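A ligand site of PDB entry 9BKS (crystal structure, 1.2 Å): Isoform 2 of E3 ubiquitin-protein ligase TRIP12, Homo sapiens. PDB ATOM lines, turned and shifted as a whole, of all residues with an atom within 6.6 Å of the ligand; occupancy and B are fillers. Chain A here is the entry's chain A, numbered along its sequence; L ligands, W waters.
Water W8 lies within hydrogen-bond range of an oxygen (O10) of the ligand and the backbone NH of Asp 15.
Water W1 lies within hydrogen-bond range of an oxygen (O2) of the ligand (2.7 Å), the side-chain carboxylate of Asp 15 (3.0 Å) and the guanidinium group of Arg 68 (3.4 Å).
Water W2 lies within hydrogen-bond range of O5 of the ligand (2.8 Å), NE2 of Gln 59 (3.0 Å) and O of Thr 66 (3.0 Å).
Water W5 bridges an oxygen (O4) of the ligand (3.0 Å) and the side-chain amide nitrogen of Asn 61 (3.4 Å).
Water W7 bridges OD2 of Asp 15 (2.7 Å) and O9 of the ligand (3.4 Å).
The side-chain hydroxyl of Thr 66 is in hydrogen-bond range of an oxygen (O1) of the ligand, 2.6 Å away.
OH of Tyr 50 lies within hydrogen-bond range of O4 of the ligand (2.6 Å).
The guanidinium group (NH1) of Arg 48 is in salt-bridge range of an oxygen (O4) of the ligand (3.96 Å).
OG1 of Thr 64 sits at hydrogen-bond distance from O1 of the ligand (2.8 Å).
The guanidinium group of Arg 68 is in salt-bridge range of an oxygen (O5) of the ligand, 2.8 Å away.
The side-chain amide nitrogen of Asn 61 lies within hydrogen-bond range of an oxygen (O4) of the ligand, at 2.8 Å.
A nitrogen (N3) of the ligand is in hydrogen-bond range of the side-chain amide oxygen (OE1) of Gln 59 (2.9 Å).
Merely in contact with the ligand: Trp 12, Tyr 22, Leu 46 and Asp 14.
Hydrophobic or aromatic side chains within 4 Å of the ligand: Trp 12, Tyr 22, Leu 46 and Tyr 50.
11 residues have an atom within 4 Å of the ligand: Trp 12, Asp 14, Tyr 22, Leu 46, Arg 48, Tyr 50, Gln 59, Asn 61, Thr 64, Thr 66 and Arg 68.
The nearest printed residue that does not touch the ligand is Thr 45 (4.3 Å).
The backbone NH of Thr 66 sits at hydrogen-bond distance from the side-chain hydroxyl of Thr 64.
The backbone NH (N) of Leu 43 is in hydrogen-bond range of the backbone carbonyl oxygen (O) of Tyr 50 (2.8 Å).
OD1 of Asn 61 sits at hydrogen-bond distance from N of Thr 64, at 3.0 Å.
The backbone NH of Gln 59 sits at hydrogen-bond distance from the backbone carbonyl oxygen of Arg 68, at 2.8 Å.
NH1 of Arg 68 is in hydrogen-bond range of O of Arg 13 (3.3 Å).
The side-chain hydroxyl (OH) of Tyr 22 is in hydrogen-bond range of the side-chain amide oxygen (OE1) of Gln 59.
O of Trp 12 is in hydrogen-bond range of N of His 20 (2.9 Å).
The side-chain carboxylate of Asp 14 sits at hydrogen-bond distance from a ring nitrogen (NE2) of His 20, at 2.7 Å.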
ATOM      1  N   TRP A  12      11.993 -17.119 -32.414  1.00  0.00           N
ATOM      2  CA  TRP A  12      12.668 -16.993 -31.132  1.00  0.00           C
ATOM      3  C   TRP A  12      13.587 -15.763 -31.167  1.00  0.00           C
ATOM      4  O   TRP A  12      14.026 -15.337 -32.238  1.00  0.00           O
ATOM      5  CB  TRP A  12      13.457 -18.275 -30.797  1.00  0.00           C
ATOM      6  CG  TRP A  12      14.472 -18.647 -31.833  1.00  0.00           C
ATOM      7  CD1 TRP A  12      14.277 -19.412 -32.947  1.00  0.00           C
ATOM      8  CD2 TRP A  12      15.845 -18.220 -31.866  1.00  0.00           C
ATOM      9  NE1 TRP A  12      15.432 -19.496 -33.671  1.00  0.00           N
ATOM     10  CE2 TRP A  12      16.404 -18.764 -33.045  1.00  0.00           C
ATOM     11  CE3 TRP A  12      16.656 -17.435 -31.036  1.00  0.00           C
ATOM     12  CZ2 TRP A  12      17.735 -18.564 -33.389  1.00  0.00           C
ATOM     13  CZ3 TRP A  12      17.966 -17.236 -31.389  1.00  0.00           C
ATOM     14  CH2 TRP A  12      18.486 -17.779 -32.546  1.00  0.00           C
ATOM     15  N   ARG A  13      13.849 -15.212 -29.989  1.00  0.00           N
ATOM     16  CA  ARG A  13      14.574 -13.945 -29.887  1.00  0.00           C
ATOM     17  C   ARG A  13      16.032 -14.151 -29.451  1.00  0.00           C
ATOM     18  O   ARG A  13      16.315 -14.829 -28.456  1.00  0.00           O
ATOM     19  CB  ARG A  13      13.855 -12.982 -28.954  1.00  0.00           C
ATOM     20  CG  ARG A  13      14.352 -11.553 -29.154  1.00  0.00           C
ATOM     21  CD  ARG A  13      13.510 -10.531 -28.451  1.00  0.00           C
ATOM     22  NE  ARG A  13      13.518 -10.757 -27.007  1.00  0.00           N
ATOM     23  CZ  ARG A  13      12.561 -10.321 -26.191  1.00  0.00           C
ATOM     24  NH1 ARG A  13      11.632  -9.505 -26.662  1.00  0.00           N
ATOM     25  NH2 ARG A  13      12.503 -10.693 -24.922  1.00  0.00           N
ATOM     26  N   ASP A  14      16.965 -13.591 -30.216  1.00  0.00           N
ATOM     27  CA  ASP A  14      18.383 -13.731 -29.944  1.00  0.00           C
ATOM     28  C   ASP A  14      18.860 -12.696 -28.916  1.00  0.00           C
ATOM     29  O   ASP A  14      18.080 -11.891 -28.430  1.00  0.00           O
ATOM     30  CB  ASP A  14      19.167 -13.697 -31.242  1.00  0.00           C
ATOM     31  CG  ASP A  14      19.340 -12.354 -31.931  1.00  0.00           C
ATOM     32  OD1 ASP A  14      19.095 -11.315 -31.290  1.00  0.00           O
ATOM     33  OD2 ASP A  14      19.679 -12.372 -33.122  1.00  0.00           O
ATOM     34  N   ASP A  15      20.158 -12.724 -28.598  1.00  0.00           N
ATOM     35  CA  ASP A  15      20.725 -11.831 -27.613  1.00  0.00           C
ATOM     36  C   ASP A  15      20.778 -10.371 -28.065  1.00  0.00           C
ATOM     37  O   ASP A  15      21.035  -9.489 -27.255  1.00  0.00           O
ATOM     38  CB  ASP A  15      22.116 -12.302 -27.203  1.00  0.00           C
ATOM     39  CG  ASP A  15      22.191 -13.696 -26.582  1.00  0.00           C
ATOM     40  OD1 ASP A  15      21.222 -14.050 -25.872  1.00  0.00           O
ATOM     41  OD2 ASP A  15      23.236 -14.368 -26.731  1.00  0.00           O
ATOM     42  N   HIS A  20      14.122 -14.664 -35.019  1.00  0.00           N
ATOM     43  CA  HIS A  20      14.517 -15.639 -36.025  1.00  0.00           C
ATOM     44  C   HIS A  20      13.423 -16.669 -36.199  1.00  0.00           C
ATOM     45  O   HIS A  20      12.932 -17.233 -35.225  1.00  0.00           O
ATOM     46  CB  HIS A  20      15.746 -16.418 -35.542  1.00  0.00           C
ATOM     47  CG  HIS A  20      16.922 -15.547 -35.370  1.00  0.00           C
ATOM     48  ND1 HIS A  20      17.872 -15.404 -36.333  1.00  0.00           N
ATOM     49  CD2 HIS A  20      17.290 -14.739 -34.389  1.00  0.00           C
ATOM     50  CE1 HIS A  20      18.792 -14.567 -35.894  1.00  0.00           C
ATOM     51  NE2 HIS A  20      18.476 -14.147 -34.697  1.00  0.00           N
ATOM     52  N   PRO A  21      13.034 -16.997 -37.449  1.00  0.00           N
ATOM     53  CA  PRO A  21      12.112 -18.113 -37.624  1.00  0.00           C
ATOM     54  C   PRO A  21      12.736 -19.442 -37.206  1.00  0.00           C
ATOM     55  O   PRO A  21      13.873 -19.730 -37.592  1.00  0.00           O
ATOM     56  CB  PRO A  21      11.805 -18.118 -39.115  1.00  0.00           C
ATOM     57  CG  PRO A  21      12.758 -17.186 -39.750  1.00  0.00           C
ATOM     58  CD  PRO A  21      13.480 -16.385 -38.706  1.00  0.00           C
ATOM     59  N   TYR A  22      11.986 -20.272 -36.469  1.00  0.00           N
ATOM     60  CA  TYR A  22      12.357 -21.667 -36.325  1.00  0.00           C
ATOM     61  C   TYR A  22      12.418 -22.317 -37.692  1.00  0.00           C
ATOM     62  O   TYR A  22      11.781 -21.832 -38.623  1.00  0.00           O
ATOM     63  CB  TYR A  22      11.302 -22.373 -35.462  1.00  0.00           C
ATOM     64  CG  TYR A  22      11.504 -22.121 -33.986  1.00  0.00           C
ATOM     65  CD1 TYR A  22      12.406 -22.875 -33.237  1.00  0.00           C
ATOM     66  CD2 TYR A  22      10.742 -21.170 -33.311  1.00  0.00           C
ATOM     67  CE1 TYR A  22      12.572 -22.654 -31.887  1.00  0.00           C
ATOM     68  CE2 TYR A  22      10.917 -20.929 -31.973  1.00  0.00           C
ATOM     69  CZ  TYR A  22      11.828 -21.685 -31.244  1.00  0.00           C
ATOM     70  OH  TYR A  22      11.972 -21.437 -29.926  1.00  0.00           O
ATOM     71  N   ASP A  26      10.319 -27.555 -37.154  1.00  0.00           N
ATOM     72  CA  ASP A  26      10.224 -27.174 -35.754  1.00  0.00           C
ATOM     73  C   ASP A  26       9.031 -26.255 -35.497  1.00  0.00           C
ATOM     74  O   ASP A  26       8.333 -26.381 -34.498  1.00  0.00           O
ATOM     75  CB  ASP A  26      11.550 -26.579 -35.296  1.00  0.00           C
ATOM     76  CG  ASP A  26      12.673 -27.613 -35.218  1.00  0.00           C
ATOM     77  OD1 ASP A  26      12.380 -28.847 -35.265  1.00  0.00           O
ATOM     78  OD2 ASP A  26      13.842 -27.211 -35.129  1.00  0.00           O
ATOM     79  N   LEU A  43      11.951 -29.854 -27.769  1.00  0.00           N
ATOM     80  CA  LEU A  43      12.380 -29.734 -29.136  1.00  0.00           C
ATOM     81  C   LEU A  43      13.894 -29.945 -29.165  1.00  0.00           C
ATOM     82  O   LEU A  43      14.595 -29.336 -28.375  1.00  0.00           O
ATOM     83  CB  LEU A  43      11.984 -28.310 -29.553  1.00  0.00           C
ATOM     84  CG  LEU A  43      12.173 -27.942 -31.028  1.00  0.00           C
ATOM     85  CD1 LEU A  43      11.030 -28.561 -31.825  1.00  0.00           C
ATOM     86  CD2 LEU A  43      12.217 -26.432 -31.233  1.00  0.00           C
ATOM     87  N   THR A  45      17.215 -29.325 -31.561  1.00  0.00           N
ATOM     88  CA  THR A  45      17.836 -28.755 -32.753  1.00  0.00           C
ATOM     89  C   THR A  45      19.289 -28.439 -32.430  1.00  0.00           C
ATOM     90  O   THR A  45      19.612 -28.060 -31.291  1.00  0.00           O
ATOM     91  CB  THR A  45      17.108 -27.516 -33.259  1.00  0.00           C
ATOM     92  OG1 THR A  45      17.669 -27.184 -34.519  1.00  0.00           O
ATOM     93  CG2 THR A  45      17.169 -26.353 -32.281  1.00  0.00           C
ATOM     94  N   LEU A  46      20.163 -28.670 -33.419  1.00  0.00           N
ATOM     95  CA  LEU A  46      21.575 -28.363 -33.334  1.00  0.00           C
ATOM     96  C   LEU A  46      22.207 -29.153 -32.197  1.00  0.00           C
ATOM     97  O   LEU A  46      23.257 -28.751 -31.709  1.00  0.00           O
ATOM     98  CB  LEU A  46      21.789 -26.861 -33.174  1.00  0.00           C
ATOM     99  CG  LEU A  46      21.304 -25.990 -34.335  1.00  0.00           C
ATOM    100  CD1 LEU A  46      21.597 -24.544 -34.015  1.00  0.00           C
ATOM    101  CD2 LEU A  46      21.954 -26.393 -35.651  1.00  0.00           C
ATOM    102  N   ARG A  48      21.001 -29.610 -29.307  1.00  0.00           N
ATOM    103  CA  ARG A  48      20.606 -29.005 -28.040  1.00  0.00           C
ATOM    104  C   ARG A  48      19.210 -29.499 -27.700  1.00  0.00           C
ATOM    105  O   ARG A  48      18.483 -30.024 -28.565  1.00  0.00           O
ATOM    106  CB  ARG A  48      20.604 -27.492 -28.182  1.00  0.00           C
ATOM    107  CG  ARG A  48      21.874 -26.954 -28.822  1.00  0.00           C
ATOM    108  CD  ARG A  48      21.606 -25.563 -29.292  1.00  0.00           C
ATOM    109  NE  ARG A  48      22.686 -25.056 -30.141  1.00  0.00           N
ATOM    110  CZ  ARG A  48      22.712 -23.807 -30.594  1.00  0.00           C
ATOM    111  NH1 ARG A  48      21.659 -23.039 -30.382  1.00  0.00           N
ATOM    112  NH2 ARG A  48      23.773 -23.325 -31.239  1.00  0.00           N
ATOM    113  N   TYR A  50      15.667 -28.095 -26.038  1.00  0.00           N
ATOM    114  CA  TYR A  50      14.920 -26.951 -25.591  1.00  0.00           C
ATOM    115  C   TYR A  50      13.551 -27.400 -25.084  1.00  0.00           C
ATOM    116  O   TYR A  50      12.905 -28.272 -25.654  1.00  0.00           O
ATOM    117  CB  TYR A  50      14.714 -25.962 -26.735  1.00  0.00           C
ATOM    118  CG  TYR A  50      16.001 -25.301 -27.204  1.00  0.00           C
ATOM    119  CD1 TYR A  50      16.668 -24.381 -26.408  1.00  0.00           C
ATOM    120  CD2 TYR A  50      16.511 -25.541 -28.466  1.00  0.00           C
ATOM    121  CE1 TYR A  50      17.828 -23.758 -26.828  1.00  0.00           C
ATOM    122  CE2 TYR A  50      17.650 -24.901 -28.906  1.00  0.00           C
ATOM    123  CZ  TYR A  50      18.328 -24.029 -28.086  1.00  0.00           C
ATOM    124  OH  TYR A  50      19.478 -23.397 -28.506  1.00  0.00           O
ATOM    125  N   GLN A  59      11.368 -20.186 -24.903  1.00  0.00           N
ATOM    126  CA  GLN A  59      12.234 -21.324 -25.176  1.00  0.00           C
ATOM    127  C   GLN A  59      13.283 -21.376 -24.080  1.00  0.00           C
ATOM    128  O   GLN A  59      13.950 -20.390 -23.841  1.00  0.00           O
ATOM    129  CB  GLN A  59      12.912 -21.107 -26.534  1.00  0.00           C
ATOM    130  CG  GLN A  59      13.954 -22.175 -26.862  1.00  0.00           C
ATOM    131  CD  GLN A  59      14.840 -21.746 -28.005  1.00  0.00           C
ATOM    132  OE1 GLN A  59      14.481 -21.898 -29.180  1.00  0.00           O
ATOM    133  NE2 GLN A  59      15.989 -21.195 -27.675  1.00  0.00           N
ATOM    134  N   ILE A  60      13.454 -22.548 -23.471  1.00  0.00           N
ATOM    135  CA  ILE A  60      14.375 -22.732 -22.368  1.00  0.00           C
ATOM    136  C   ILE A  60      15.414 -23.775 -22.757  1.00  0.00           C
ATOM    137  O   ILE A  60      15.066 -24.920 -23.060  1.00  0.00           O
ATOM    138  CB  ILE A  60      13.637 -23.137 -21.083  1.00  0.00           C
ATOM    139  CG1 ILE A  60      12.537 -22.147 -20.726  1.00  0.00           C
ATOM    140  CG2 ILE A  60      14.629 -23.316 -19.943  1.00  0.00           C
ATOM    141  CD1 ILE A  60      11.515 -22.671 -19.728  1.00  0.00           C
ATOM    142  N   ASN A  61      16.703 -23.411 -22.681  1.00  0.00           N
ATOM    143  CA  ASN A  61      17.770 -24.370 -22.898  1.00  0.00           C
ATOM    144  C   ASN A  61      17.898 -25.210 -21.641  1.00  0.00           C
ATOM    145  O   ASN A  61      18.184 -24.658 -20.575  1.00  0.00           O
ATOM    146  CB  ASN A  61      19.051 -23.640 -23.262  1.00  0.00           C
ATOM    147  CG  ASN A  61      20.203 -24.582 -23.545  1.00  0.00           C
ATOM    148  OD1 ASN A  61      20.418 -25.542 -22.806  1.00  0.00           O
ATOM    149  ND2 ASN A  61      20.987 -24.317 -24.580  1.00  0.00           N
ATOM    150  N   THR A  64      21.669 -24.949 -20.093  1.00  0.00           N
ATOM    151  CA  THR A  64      22.253 -23.686 -19.632  1.00  0.00           C
ATOM    152  C   THR A  64      21.282 -22.876 -18.775  1.00  0.00           C
ATOM    153  O   THR A  64      21.714 -21.968 -18.066  1.00  0.00           O
ATOM    154  CB  THR A  64      22.699 -22.817 -20.799  1.00  0.00           C
ATOM    155  OG1 THR A  64      21.535 -22.343 -21.472  1.00  0.00           O
ATOM    156  CG2 THR A  64      23.673 -23.505 -21.747  1.00  0.00           C
ATOM    157  N   GLY A  65      19.978 -23.132 -18.890  1.00  0.00           N
ATOM    158  CA  GLY A  65      18.980 -22.344 -18.180  1.00  0.00           C
ATOM    159  C   GLY A  65      18.603 -21.031 -18.859  1.00  0.00           C
ATOM    160  O   GLY A  65      17.778 -20.292 -18.315  1.00  0.00           O
ATOM    161  N   THR A  66      19.149 -20.763 -20.044  1.00  0.00           N
ATOM    162  CA  THR A  66      18.782 -19.531 -20.737  1.00  0.00           C
ATOM    163  C   THR A  66      17.363 -19.646 -21.310  1.00  0.00           C
ATOM    164  O   THR A  66      17.051 -20.603 -22.031  1.00  0.00           O
ATOM    165  CB  THR A  66      19.772 -19.228 -21.846  1.00  0.00           C
ATOM    166  OG1 THR A  66      21.040 -18.944 -21.249  1.00  0.00           O
ATOM    167  CG2 THR A  66      19.358 -18.040 -22.694  1.00  0.00           C
ATOM    168  N   ALA A  67      16.560 -18.626 -21.010  1.00  0.00           N
ATOM    169  CA  ALA A  67      15.200 -18.483 -21.516  1.00  0.00           C
ATOM    170  C   ALA A  67      15.169 -17.351 -22.540  1.00  0.00           C
ATOM    171  O   ALA A  67      15.714 -16.278 -22.302  1.00  0.00           O
ATOM    172  CB  ALA A  67      14.232 -18.172 -20.378  1.00  0.00           C
ATOM    173  N   ARG A  68      14.514 -17.615 -23.661  1.00  0.00           N
ATOM    174  CA  ARG A  68      14.363 -16.651 -24.746  1.00  0.00           C
ATOM    175  C   ARG A  68      12.890 -16.539 -25.113  1.00  0.00           C
ATOM    176  O   ARG A  68      12.173 -17.531 -25.158  1.00  0.00           O
ATOM    177  CB  ARG A  68      15.137 -17.136 -26.001  1.00  0.00           C
ATOM    178  CG  ARG A  68      16.633 -17.257 -25.765  1.00  0.00           C
ATOM    179  CD  ARG A  68      17.371 -17.769 -26.966  1.00  0.00           C
ATOM    180  NE  ARG A  68      18.807 -17.789 -26.705  1.00  0.00           N
ATOM    181  CZ  ARG A  68      19.596 -16.720 -26.600  1.00  0.00           C
ATOM    182  NH1 ARG A  68      19.119 -15.533 -26.933  1.00  0.00           N
ATOM    183  NH2 ARG A  68      20.878 -16.847 -26.252  1.00  0.00           N
HETATM  184  P1  LIG L   1      23.048 -19.919 -24.184  1.00  0.00           P
HETATM  185  O1  LIG L   1      22.747 -20.221 -22.739  1.00  0.00           O
HETATM  186  O2  LIG L   1      22.583 -18.558 -24.612  1.00  0.00           O
HETATM  187  O3  LIG L   1      24.466 -20.188 -24.535  1.00  0.00           O
HETATM  188  P2  LIG L   1      21.051 -20.897 -26.125  1.00  0.00           P
HETATM  189  O4  LIG L   1      20.841 -22.302 -26.574  1.00  0.00           O
HETATM  190  O5  LIG L   1      19.850 -20.123 -25.675  1.00  0.00           O
HETATM  191  O6  LIG L   1      22.172 -20.985 -24.999  1.00  0.00           O
HETATM  192  O7  LIG L   1      21.698 -20.034 -27.302  1.00  0.00           O
HETATM  193  C1  LIG L   1      22.969 -20.452 -27.834  1.00  0.00           C
HETATM  194  C2  LIG L   1      23.199 -19.802 -29.184  1.00  0.00           C
HETATM  195  O8  LIG L   1      22.278 -20.369 -30.147  1.00  0.00           O
HETATM  196  C3  LIG L   1      23.009 -18.289 -29.286  1.00  0.00           C
HETATM  197  O9  LIG L   1      23.817 -17.764 -30.343  1.00  0.00           O
HETATM  198  C4  LIG L   1      21.535 -18.179 -29.673  1.00  0.00           C
HETATM  199  O10 LIG L   1      21.238 -16.999 -30.396  1.00  0.00           O
HETATM  200  C5  LIG L   1      21.339 -19.409 -30.569  1.00  0.00           C
HETATM  201  N1  LIG L   1      20.000 -19.983 -30.505  1.00  0.00           N
HETATM  202  C6  LIG L   1      19.101 -19.949 -29.469  1.00  0.00           C
HETATM  203  N2  LIG L   1      17.986 -20.585 -29.733  1.00  0.00           N
HETATM  204  C7  LIG L   1      18.160 -21.094 -31.007  1.00  0.00           C
HETATM  205  C8  LIG L   1      17.336 -21.842 -31.869  1.00  0.00           C
HETATM  206  N3  LIG L   1      16.108 -22.223 -31.546  1.00  0.00           N
HETATM  207  N4  LIG L   1      17.840 -22.179 -33.083  1.00  0.00           N
HETATM  208  C9  LIG L   1      19.080 -21.787 -33.398  1.00  0.00           C
HETATM  209  N5  LIG L   1      19.936 -21.071 -32.685  1.00  0.00           N
HETATM  210  C10 LIG L   1      19.412 -20.755 -31.478  1.00  0.00           C
HETATM  211  O   HOH W   1      24.309 -17.166 -26.237  1.00  0.00           O
HETATM  212  O   HOH W   2      17.230 -20.757 -25.021  1.00  0.00           O
HETATM  213  O   HOH W   3      16.668 -23.096 -35.341  1.00  0.00           O
HETATM  214  O   HOH W   4      21.977 -16.802 -32.900  1.00  0.00           O
HETATM  215  O   HOH W   5      23.404 -23.787 -26.864  1.00  0.00           O
HETATM  216  O   HOH W   6      25.390 -22.528 -25.427  1.00  0.00           O
HETATM  217  O   HOH W   7      24.586 -14.683 -29.013  1.00  0.00           O
HETATM  218  O   HOH W   8      21.967 -14.695 -29.494  1.00  0.00           O
